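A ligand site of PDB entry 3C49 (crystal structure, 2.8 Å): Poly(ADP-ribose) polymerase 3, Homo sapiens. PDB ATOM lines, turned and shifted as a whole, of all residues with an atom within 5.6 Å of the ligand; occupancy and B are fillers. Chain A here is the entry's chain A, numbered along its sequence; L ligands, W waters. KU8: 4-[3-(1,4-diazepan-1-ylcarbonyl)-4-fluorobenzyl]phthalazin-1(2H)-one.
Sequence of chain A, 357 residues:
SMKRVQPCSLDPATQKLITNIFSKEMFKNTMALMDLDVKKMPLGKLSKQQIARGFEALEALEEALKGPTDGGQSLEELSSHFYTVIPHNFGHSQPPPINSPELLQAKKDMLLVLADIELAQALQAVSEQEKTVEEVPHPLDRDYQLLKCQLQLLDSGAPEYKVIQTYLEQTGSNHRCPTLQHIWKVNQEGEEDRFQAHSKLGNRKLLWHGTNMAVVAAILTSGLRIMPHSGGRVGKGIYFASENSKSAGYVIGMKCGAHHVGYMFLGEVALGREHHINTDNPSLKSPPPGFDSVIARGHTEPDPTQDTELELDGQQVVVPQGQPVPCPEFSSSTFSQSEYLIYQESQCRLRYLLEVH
NZ of Lys 246 is in salt-bridge range of OE2 of Glu 339, at 3.0 Å. The side-chain hydroxyl (OG) of Ser 230 lies within hydrogen-bond range of the backbone carbonyl oxygen (O) of Met 227 (2.6 Å). ND1 of His 209 lies within hydrogen-bond range of O of Tyr 239, at 2.6 Å. The side-chain hydroxyl of Ser 247 is in hydrogen-bond range of the backbone carbonyl oxygen of Trp 208, 3.3 Å away. O of Gly 235 is in hydrogen-bond range of OH of Tyr 239 (2.7 Å). The side-chain amino group of Lys 246 is in hydrogen-bond range of the side-chain hydroxyl of Tyr 250 (2.8 Å). N of Gly 210 lies close to OG of Ser 247, 3.4 Å away.
Water W1 bridges N1R of the ligand (2.7 Å) and NH2 of Arg 225 (3.0 Å).
CE1 of His 209 touches O1A of the ligand, 2.8 Å away. Ser 230 touches the ligand (CB to F1C, 3.8 Å). Gly 231 touches the ligand (O to C1G, 3.3 Å). Gly 237 touches the ligand. CG2 of Ile 238 touches C1O of the ligand, 3.9 Å away. O of Phe 240 touches C1E of the ligand, 3.9 Å away. Lys 246 touches the ligand (CE to C1D, 3.7 Å). Tyr 250 touches the ligand. CG of Glu 339 touches C1D of the ligand, 3.5 Å away. Hydrophobic or aromatic side chains within 4 Å of the ligand: His 209, Ile 238, Tyr 239 and Tyr 250. Of the 24 residues printed, 13 come within 4 Å of the ligand. The nearest printed residue that does not touch the ligand is Ala 241 (4.02 Å).
O of Gly 210 is in hydrogen-bond range of N1S of the ligand, at 2.9 Å. An oxygen (O1B) of the ligand sits at hydrogen-bond distance from the backbone NH (N) of Gly 210 (2.6 Å). OG of Ser 247 is in hydrogen-bond range of O1B of the ligand (3.0 Å). The backbone carbonyl oxygen (O) of Arg 225 lies close to a nitrogen (N1R) of the ligand, 3.4 Å away. O1A of the ligand is in hydrogen-bond range of N of Tyr 239, 2.9 Å away.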
ATOM      1  N   LEU A 112     -12.086   9.717  25.390  1.00  0.00           N
ATOM      2  CA  LEU A 112     -11.764  10.126  24.030  1.00  0.00           C
ATOM      3  C   LEU A 112     -10.699  11.203  24.011  1.00  0.00           C
ATOM      4  O   LEU A 112      -9.812  11.206  23.149  1.00  0.00           O
ATOM      5  CB  LEU A 112     -13.027  10.609  23.305  1.00  0.00           C
ATOM      6  CG  LEU A 112     -13.975   9.523  22.816  1.00  0.00           C
ATOM      7  CD1 LEU A 112     -15.262  10.135  22.247  1.00  0.00           C
ATOM      8  CD2 LEU A 112     -13.301   8.635  21.773  1.00  0.00           C
ATOM      9  N   TRP A 208     -16.802  26.894  12.256  1.00  0.00           N
ATOM     10  CA  TRP A 208     -15.953  26.882  13.442  1.00  0.00           C
ATOM     11  C   TRP A 208     -15.957  25.513  14.110  1.00  0.00           C
ATOM     12  O   TRP A 208     -16.952  24.798  14.068  1.00  0.00           O
ATOM     13  CB  TRP A 208     -16.421  27.924  14.455  1.00  0.00           C
ATOM     14  CG  TRP A 208     -16.232  29.340  14.006  1.00  0.00           C
ATOM     15  CD1 TRP A 208     -17.184  30.178  13.530  1.00  0.00           C
ATOM     16  CD2 TRP A 208     -15.013  30.076  14.022  1.00  0.00           C
ATOM     17  NE1 TRP A 208     -16.637  31.399  13.226  1.00  0.00           N
ATOM     18  CE2 TRP A 208     -15.301  31.369  13.523  1.00  0.00           C
ATOM     19  CE3 TRP A 208     -13.701  29.786  14.391  1.00  0.00           C
ATOM     20  CZ2 TRP A 208     -14.323  32.353  13.387  1.00  0.00           C
ATOM     21  CZ3 TRP A 208     -12.731  30.763  14.268  1.00  0.00           C
ATOM     22  CH2 TRP A 208     -13.043  32.027  13.770  1.00  0.00           C
ATOM     23  N   HIS A 209     -14.836  25.168  14.724  1.00  0.00           N
ATOM     24  CA  HIS A 209     -14.772  23.977  15.560  1.00  0.00           C
ATOM     25  C   HIS A 209     -13.931  24.236  16.806  1.00  0.00           C
ATOM     26  O   HIS A 209     -12.698  24.226  16.756  1.00  0.00           O
ATOM     27  CB  HIS A 209     -14.252  22.761  14.791  1.00  0.00           C
ATOM     28  CG  HIS A 209     -14.372  21.480  15.541  1.00  0.00           C
ATOM     29  ND1 HIS A 209     -15.582  20.828  15.715  1.00  0.00           N
ATOM     30  CD2 HIS A 209     -13.448  20.721  16.175  1.00  0.00           C
ATOM     31  CE1 HIS A 209     -15.390  19.734  16.426  1.00  0.00           C
ATOM     32  NE2 HIS A 209     -14.113  19.645  16.719  1.00  0.00           N
ATOM     33  N   GLY A 210     -14.603  24.462  17.925  1.00  0.00           N
ATOM     34  CA  GLY A 210     -13.943  24.708  19.196  1.00  0.00           C
ATOM     35  C   GLY A 210     -13.439  23.431  19.829  1.00  0.00           C
ATOM     36  O   GLY A 210     -14.094  22.393  19.774  1.00  0.00           O
ATOM     37  N   THR A 211     -12.269  23.515  20.446  1.00  0.00           N
ATOM     38  CA  THR A 211     -11.593  22.335  20.965  1.00  0.00           C
ATOM     39  C   THR A 211     -10.701  22.719  22.141  1.00  0.00           C
ATOM     40  O   THR A 211     -10.122  23.803  22.152  1.00  0.00           O
ATOM     41  CB  THR A 211     -10.713  21.703  19.882  1.00  0.00           C
ATOM     42  OG1 THR A 211      -9.844  20.731  20.469  1.00  0.00           O
ATOM     43  CG2 THR A 211      -9.861  22.777  19.201  1.00  0.00           C
ATOM     44  N   ILE A 219      -5.384  16.557  16.314  1.00  0.00           N
ATOM     45  CA  ILE A 219      -6.153  16.987  15.136  1.00  0.00           C
ATOM     46  C   ILE A 219      -5.247  17.473  14.010  1.00  0.00           C
ATOM     47  O   ILE A 219      -5.487  17.184  12.848  1.00  0.00           O
ATOM     48  CB  ILE A 219      -7.172  18.083  15.462  1.00  0.00           C
ATOM     49  CG1 ILE A 219      -8.226  17.563  16.442  1.00  0.00           C
ATOM     50  CG2 ILE A 219      -7.840  18.568  14.195  1.00  0.00           C
ATOM     51  CD1 ILE A 219      -9.279  18.594  16.788  1.00  0.00           C
ATOM     52  N   LEU A 224      -9.912  15.861  11.724  1.00  0.00           N
ATOM     53  CA  LEU A 224     -11.128  15.608  12.476  1.00  0.00           C
ATOM     54  C   LEU A 224     -11.648  14.209  12.182  1.00  0.00           C
ATOM     55  O   LEU A 224     -11.688  13.774  11.025  1.00  0.00           O
ATOM     56  CB  LEU A 224     -12.185  16.656  12.170  1.00  0.00           C
ATOM     57  CG  LEU A 224     -11.839  18.050  12.706  1.00  0.00           C
ATOM     58  CD1 LEU A 224     -12.894  19.062  12.333  1.00  0.00           C
ATOM     59  CD2 LEU A 224     -11.647  18.000  14.213  1.00  0.00           C
ATOM     60  N   ARG A 225     -12.038  13.500  13.244  1.00  0.00           N
ATOM     61  CA  ARG A 225     -12.375  12.090  13.139  1.00  0.00           C
ATOM     62  C   ARG A 225     -13.695  11.777  13.824  1.00  0.00           C
ATOM     63  O   ARG A 225     -13.961  12.232  14.935  1.00  0.00           O
ATOM     64  CB  ARG A 225     -11.267  11.236  13.770  1.00  0.00           C
ATOM     65  CG  ARG A 225      -9.914  11.357  13.108  1.00  0.00           C
ATOM     66  CD  ARG A 225      -8.807  11.263  14.145  1.00  0.00           C
ATOM     67  NE  ARG A 225      -8.603  12.549  14.801  1.00  0.00           N
ATOM     68  CZ  ARG A 225      -8.155  12.701  16.047  1.00  0.00           C
ATOM     69  NH1 ARG A 225      -7.880  11.640  16.794  1.00  0.00           N
ATOM     70  NH2 ARG A 225      -8.001  13.915  16.551  1.00  0.00           N
ATOM     71  N   ILE A 226     -14.524  10.982  13.161  1.00  0.00           N
ATOM     72  CA  ILE A 226     -15.736  10.482  13.775  1.00  0.00           C
ATOM     73  C   ILE A 226     -15.369   9.315  14.670  1.00  0.00           C
ATOM     74  O   ILE A 226     -15.071   8.220  14.190  1.00  0.00           O
ATOM     75  CB  ILE A 226     -16.763  10.041  12.717  1.00  0.00           C
ATOM     76  CG1 ILE A 226     -17.254  11.253  11.937  1.00  0.00           C
ATOM     77  CG2 ILE A 226     -17.922   9.300  13.370  1.00  0.00           C
ATOM     78  CD1 ILE A 226     -18.023  10.907  10.692  1.00  0.00           C
ATOM     79  N   MET A 227     -15.359   9.560  15.980  1.00  0.00           N
ATOM     80  CA  MET A 227     -14.907   8.568  16.943  1.00  0.00           C
ATOM     81  C   MET A 227     -16.038   7.691  17.460  1.00  0.00           C
ATOM     82  O   MET A 227     -17.168   8.148  17.611  1.00  0.00           O
ATOM     83  CB  MET A 227     -14.206   9.252  18.121  1.00  0.00           C
ATOM     84  CG  MET A 227     -12.907   9.958  17.758  1.00  0.00           C
ATOM     85  SD  MET A 227     -11.722   8.865  16.952  1.00  0.00           S
ATOM     86  CE  MET A 227     -11.391   7.683  18.267  1.00  0.00           C
ATOM     87  N   SER A 230     -18.606   8.514  20.751  1.00  0.00           N
ATOM     88  CA  SER A 230     -18.883   9.943  20.808  1.00  0.00           C
ATOM     89  C   SER A 230     -20.324  10.216  20.421  1.00  0.00           C
ATOM     90  O   SER A 230     -20.762   9.891  19.314  1.00  0.00           O
ATOM     91  CB  SER A 230     -17.933  10.709  19.885  1.00  0.00           C
ATOM     92  OG  SER A 230     -18.158  10.384  18.528  1.00  0.00           O
ATOM     93  N   GLY A 231     -21.079  10.822  21.333  1.00  0.00           N
ATOM     94  CA  GLY A 231     -22.463  11.163  21.076  1.00  0.00           C
ATOM     95  C   GLY A 231     -22.692  12.651  21.183  1.00  0.00           C
ATOM     96  O   GLY A 231     -21.818  13.398  21.604  1.00  0.00           O
ATOM     97  N   GLY A 232     -23.889  13.092  20.787  1.00  0.00           N
ATOM     98  CA  GLY A 232     -24.241  14.495  20.846  1.00  0.00           C
ATOM     99  C   GLY A 232     -25.723  14.708  20.587  1.00  0.00           C
ATOM    100  O   GLY A 232     -26.477  13.751  20.412  1.00  0.00           O
ATOM    101  N   GLY A 235     -26.388  13.268  17.135  1.00  0.00           N
ATOM    102  CA  GLY A 235     -25.865  11.959  16.816  1.00  0.00           C
ATOM    103  C   GLY A 235     -24.363  11.878  16.665  1.00  0.00           C
ATOM    104  O   GLY A 235     -23.620  12.710  17.193  1.00  0.00           O
ATOM    105  N   GLY A 237     -21.326  12.285  14.628  1.00  0.00           N
ATOM    106  CA  GLY A 237     -20.647  12.876  13.492  1.00  0.00           C
ATOM    107  C   GLY A 237     -19.645  13.934  13.911  1.00  0.00           C
ATOM    108  O   GLY A 237     -19.217  13.983  15.069  1.00  0.00           O
ATOM    109  N   ILE A 238     -19.246  14.782  12.965  1.00  0.00           N
ATOM    110  CA  ILE A 238     -18.337  15.879  13.262  1.00  0.00           C
ATOM    111  C   ILE A 238     -19.138  17.183  13.344  1.00  0.00           C
ATOM    112  O   ILE A 238     -19.832  17.549  12.404  1.00  0.00           O
ATOM    113  CB  ILE A 238     -17.222  15.997  12.206  1.00  0.00           C
ATOM    114  CG1 ILE A 238     -16.571  14.630  11.984  1.00  0.00           C
ATOM    115  CG2 ILE A 238     -16.191  17.014  12.637  1.00  0.00           C
ATOM    116  CD1 ILE A 238     -15.559  14.616  10.854  1.00  0.00           C
ATOM    117  N   TYR A 239     -19.035  17.855  14.479  1.00  0.00           N
ATOM    118  CA  TYR A 239     -19.839  19.040  14.755  1.00  0.00           C
ATOM    119  C   TYR A 239     -19.143  20.346  14.376  1.00  0.00           C
ATOM    120  O   TYR A 239     -17.956  20.532  14.632  1.00  0.00           O
ATOM    121  CB  TYR A 239     -20.216  19.083  16.242  1.00  0.00           C
ATOM    122  CG  TYR A 239     -21.241  18.064  16.660  1.00  0.00           C
ATOM    123  CD1 TYR A 239     -22.513  18.451  17.048  1.00  0.00           C
ATOM    124  CD2 TYR A 239     -20.942  16.700  16.667  1.00  0.00           C
ATOM    125  CE1 TYR A 239     -23.462  17.523  17.438  1.00  0.00           C
ATOM    126  CE2 TYR A 239     -21.881  15.771  17.056  1.00  0.00           C
ATOM    127  CZ  TYR A 239     -23.139  16.188  17.445  1.00  0.00           C
ATOM    128  OH  TYR A 239     -24.077  15.268  17.831  1.00  0.00           O
ATOM    129  N   PHE A 240     -19.906  21.259  13.787  1.00  0.00           N
ATOM    130  CA  PHE A 240     -19.414  22.590  13.452  1.00  0.00           C
ATOM    131  C   PHE A 240     -20.442  23.642  13.809  1.00  0.00           C
ATOM    132  O   PHE A 240     -21.632  23.366  13.878  1.00  0.00           O
ATOM    133  CB  PHE A 240     -19.073  22.682  11.966  1.00  0.00           C
ATOM    134  CG  PHE A 240     -17.948  21.792  11.541  1.00  0.00           C
ATOM    135  CD1 PHE A 240     -16.675  22.294  11.404  1.00  0.00           C
ATOM    136  CD2 PHE A 240     -18.177  20.453  11.280  1.00  0.00           C
ATOM    137  CE1 PHE A 240     -15.628  21.469  11.015  1.00  0.00           C
ATOM    138  CE2 PHE A 240     -17.142  19.627  10.883  1.00  0.00           C
ATOM    139  CZ  PHE A 240     -15.866  20.141  10.755  1.00  0.00           C
ATOM    140  N   ALA A 241     -19.972  24.860  14.059  1.00  0.00           N
ATOM    141  CA  ALA A 241     -20.853  25.980  14.346  1.00  0.00           C
ATOM    142  C   ALA A 241     -20.577  27.131  13.387  1.00  0.00           C
ATOM    143  O   ALA A 241     -19.432  27.328  12.957  1.00  0.00           O
ATOM    144  CB  ALA A 241     -20.682  26.427  15.775  1.00  0.00           C
ATOM    145  N   LYS A 246     -20.587  29.804  19.812  1.00  0.00           N
ATOM    146  CA  LYS A 246     -21.013  28.435  20.088  1.00  0.00           C
ATOM    147  C   LYS A 246     -19.804  27.514  20.268  1.00  0.00           C
ATOM    148  O   LYS A 246     -19.739  26.740  21.225  1.00  0.00           O
ATOM    149  CB  LYS A 246     -21.919  27.931  18.962  1.00  0.00           C
ATOM    150  CG  LYS A 246     -22.212  26.431  19.013  1.00  0.00           C
ATOM    151  CD  LYS A 246     -23.073  26.038  20.204  1.00  0.00           C
ATOM    152  CE  LYS A 246     -23.553  24.592  20.078  1.00  0.00           C
ATOM    153  NZ  LYS A 246     -24.172  24.060  21.314  1.00  0.00           N
ATOM    154  N   SER A 247     -18.847  27.612  19.349  1.00  0.00           N
ATOM    155  CA  SER A 247     -17.646  26.783  19.396  1.00  0.00           C
ATOM    156  C   SER A 247     -16.711  27.138  20.547  1.00  0.00           C
ATOM    157  O   SER A 247     -16.062  26.268  21.111  1.00  0.00           O
ATOM    158  CB  SER A 247     -16.892  26.854  18.068  1.00  0.00           C
ATOM    159  OG  SER A 247     -17.505  26.024  17.088  1.00  0.00           O
ATOM    160  N   TYR A 250     -16.572  25.460  23.922  1.00  0.00           N
ATOM    161  CA  TYR A 250     -15.864  24.183  24.066  1.00  0.00           C
ATOM    162  C   TYR A 250     -14.344  24.377  24.094  1.00  0.00           C
ATOM    163  O   TYR A 250     -13.599  23.405  24.102  1.00  0.00           O
ATOM    164  CB  TYR A 250     -16.246  23.231  22.931  1.00  0.00           C
ATOM    165  CG  TYR A 250     -17.726  23.086  22.726  1.00  0.00           C
ATOM    166  CD1 TYR A 250     -18.441  22.060  23.344  1.00  0.00           C
ATOM    167  CD2 TYR A 250     -18.428  23.964  21.910  1.00  0.00           C
ATOM    168  CE1 TYR A 250     -19.813  21.924  23.164  1.00  0.00           C
ATOM    169  CE2 TYR A 250     -19.791  23.834  21.716  1.00  0.00           C
ATOM    170  CZ  TYR A 250     -20.472  22.819  22.344  1.00  0.00           C
ATOM    171  OH  TYR A 250     -21.834  22.699  22.148  1.00  0.00           O
ATOM    172  N   SER A 338     -27.085  27.234  15.762  1.00  0.00           N
ATOM    173  CA  SER A 338     -26.972  26.145  14.801  1.00  0.00           C
ATOM    174  C   SER A 338     -25.847  25.145  15.112  1.00  0.00           C
ATOM    175  O   SER A 338     -24.806  25.517  15.647  1.00  0.00           O
ATOM    176  CB  SER A 338     -26.791  26.694  13.382  1.00  0.00           C
ATOM    177  OG  SER A 338     -28.028  27.127  12.850  1.00  0.00           O
ATOM    178  N   GLU A 339     -26.076  23.888  14.761  1.00  0.00           N
ATOM    179  CA  GLU A 339     -25.050  22.857  14.861  1.00  0.00           C
ATOM    180  C   GLU A 339     -25.009  22.073  13.548  1.00  0.00           C
ATOM    181  O   GLU A 339     -25.934  21.340  13.220  1.00  0.00           O
ATOM    182  CB  GLU A 339     -25.318  21.909  16.039  1.00  0.00           C
ATOM    183  CG  GLU A 339     -24.972  22.520  17.380  1.00  0.00           C
ATOM    184  CD  GLU A 339     -25.365  21.643  18.562  1.00  0.00           C
ATOM    185  OE1 GLU A 339     -25.216  20.411  18.472  1.00  0.00           O
ATOM    186  OE2 GLU A 339     -25.803  22.203  19.586  1.00  0.00           O
HETATM  187  C1N KU8 L   1     -16.556  14.396  18.106  1.00  0.00           C
HETATM  188  C1K KU8 L   1     -15.273  14.227  18.949  1.00  0.00           C
HETATM  189  C1L KU8 L   1     -13.991  13.972  18.152  1.00  0.00           C
HETATM  190  N1R KU8 L   1     -13.327  14.783  17.120  1.00  0.00           N
HETATM  191  C1M KU8 L   1     -14.186  15.045  15.946  1.00  0.00           C
HETATM  192  C1O KU8 L   1     -15.402  15.884  16.257  1.00  0.00           C
HETATM  193  N2B KU8 L   1     -16.430  15.542  17.214  1.00  0.00           N
HETATM  194  C1T KU8 L   1     -17.283  16.555  17.402  1.00  0.00           C
HETATM  195  O1A KU8 L   1     -17.193  17.591  16.741  1.00  0.00           O
HETATM  196  C1W KU8 L   1     -18.336  16.499  18.525  1.00  0.00           C
HETATM  197  C1J KU8 L   1     -18.439  17.721  19.172  1.00  0.00           C
HETATM  198  C1V KU8 L   1     -18.929  15.410  19.169  1.00  0.00           C
HETATM  199  F1C KU8 L   1     -18.888  14.174  18.623  1.00  0.00           F
HETATM  200  C1G KU8 L   1     -19.803  15.595  20.230  1.00  0.00           C
HETATM  201  C1F KU8 L   1     -19.948  16.846  20.808  1.00  0.00           C
HETATM  202  C1U KU8 L   1     -19.262  17.922  20.270  1.00  0.00           C
HETATM  203  C1P KU8 L   1     -19.419  19.292  20.920  1.00  0.00           C
HETATM  204  C1X KU8 L   1     -18.775  20.412  20.110  1.00  0.00           C
HETATM  205  C1Z KU8 L   1     -19.539  21.248  19.317  1.00  0.00           C
HETATM  206  C1H KU8 L   1     -20.917  21.043  19.237  1.00  0.00           C
HETATM  207  C1D KU8 L   1     -21.682  21.877  18.434  1.00  0.00           C
HETATM  208  C1E KU8 L   1     -21.081  22.897  17.719  1.00  0.00           C
HETATM  209  C1I KU8 L   1     -19.704  23.093  17.801  1.00  0.00           C
HETATM  210  C2A KU8 L   1     -18.938  22.259  18.603  1.00  0.00           C
HETATM  211  C1Y KU8 L   1     -17.566  22.413  18.727  1.00  0.00           C
HETATM  212  O1B KU8 L   1     -16.969  23.303  18.113  1.00  0.00           O
HETATM  213  N1S KU8 L   1     -16.873  21.519  19.560  1.00  0.00           N
HETATM  214  N1Q KU8 L   1     -17.448  20.621  20.191  1.00  0.00           N
HETATM  215  O   HOH W   1     -10.863  14.630  16.115  1.00  0.00           O
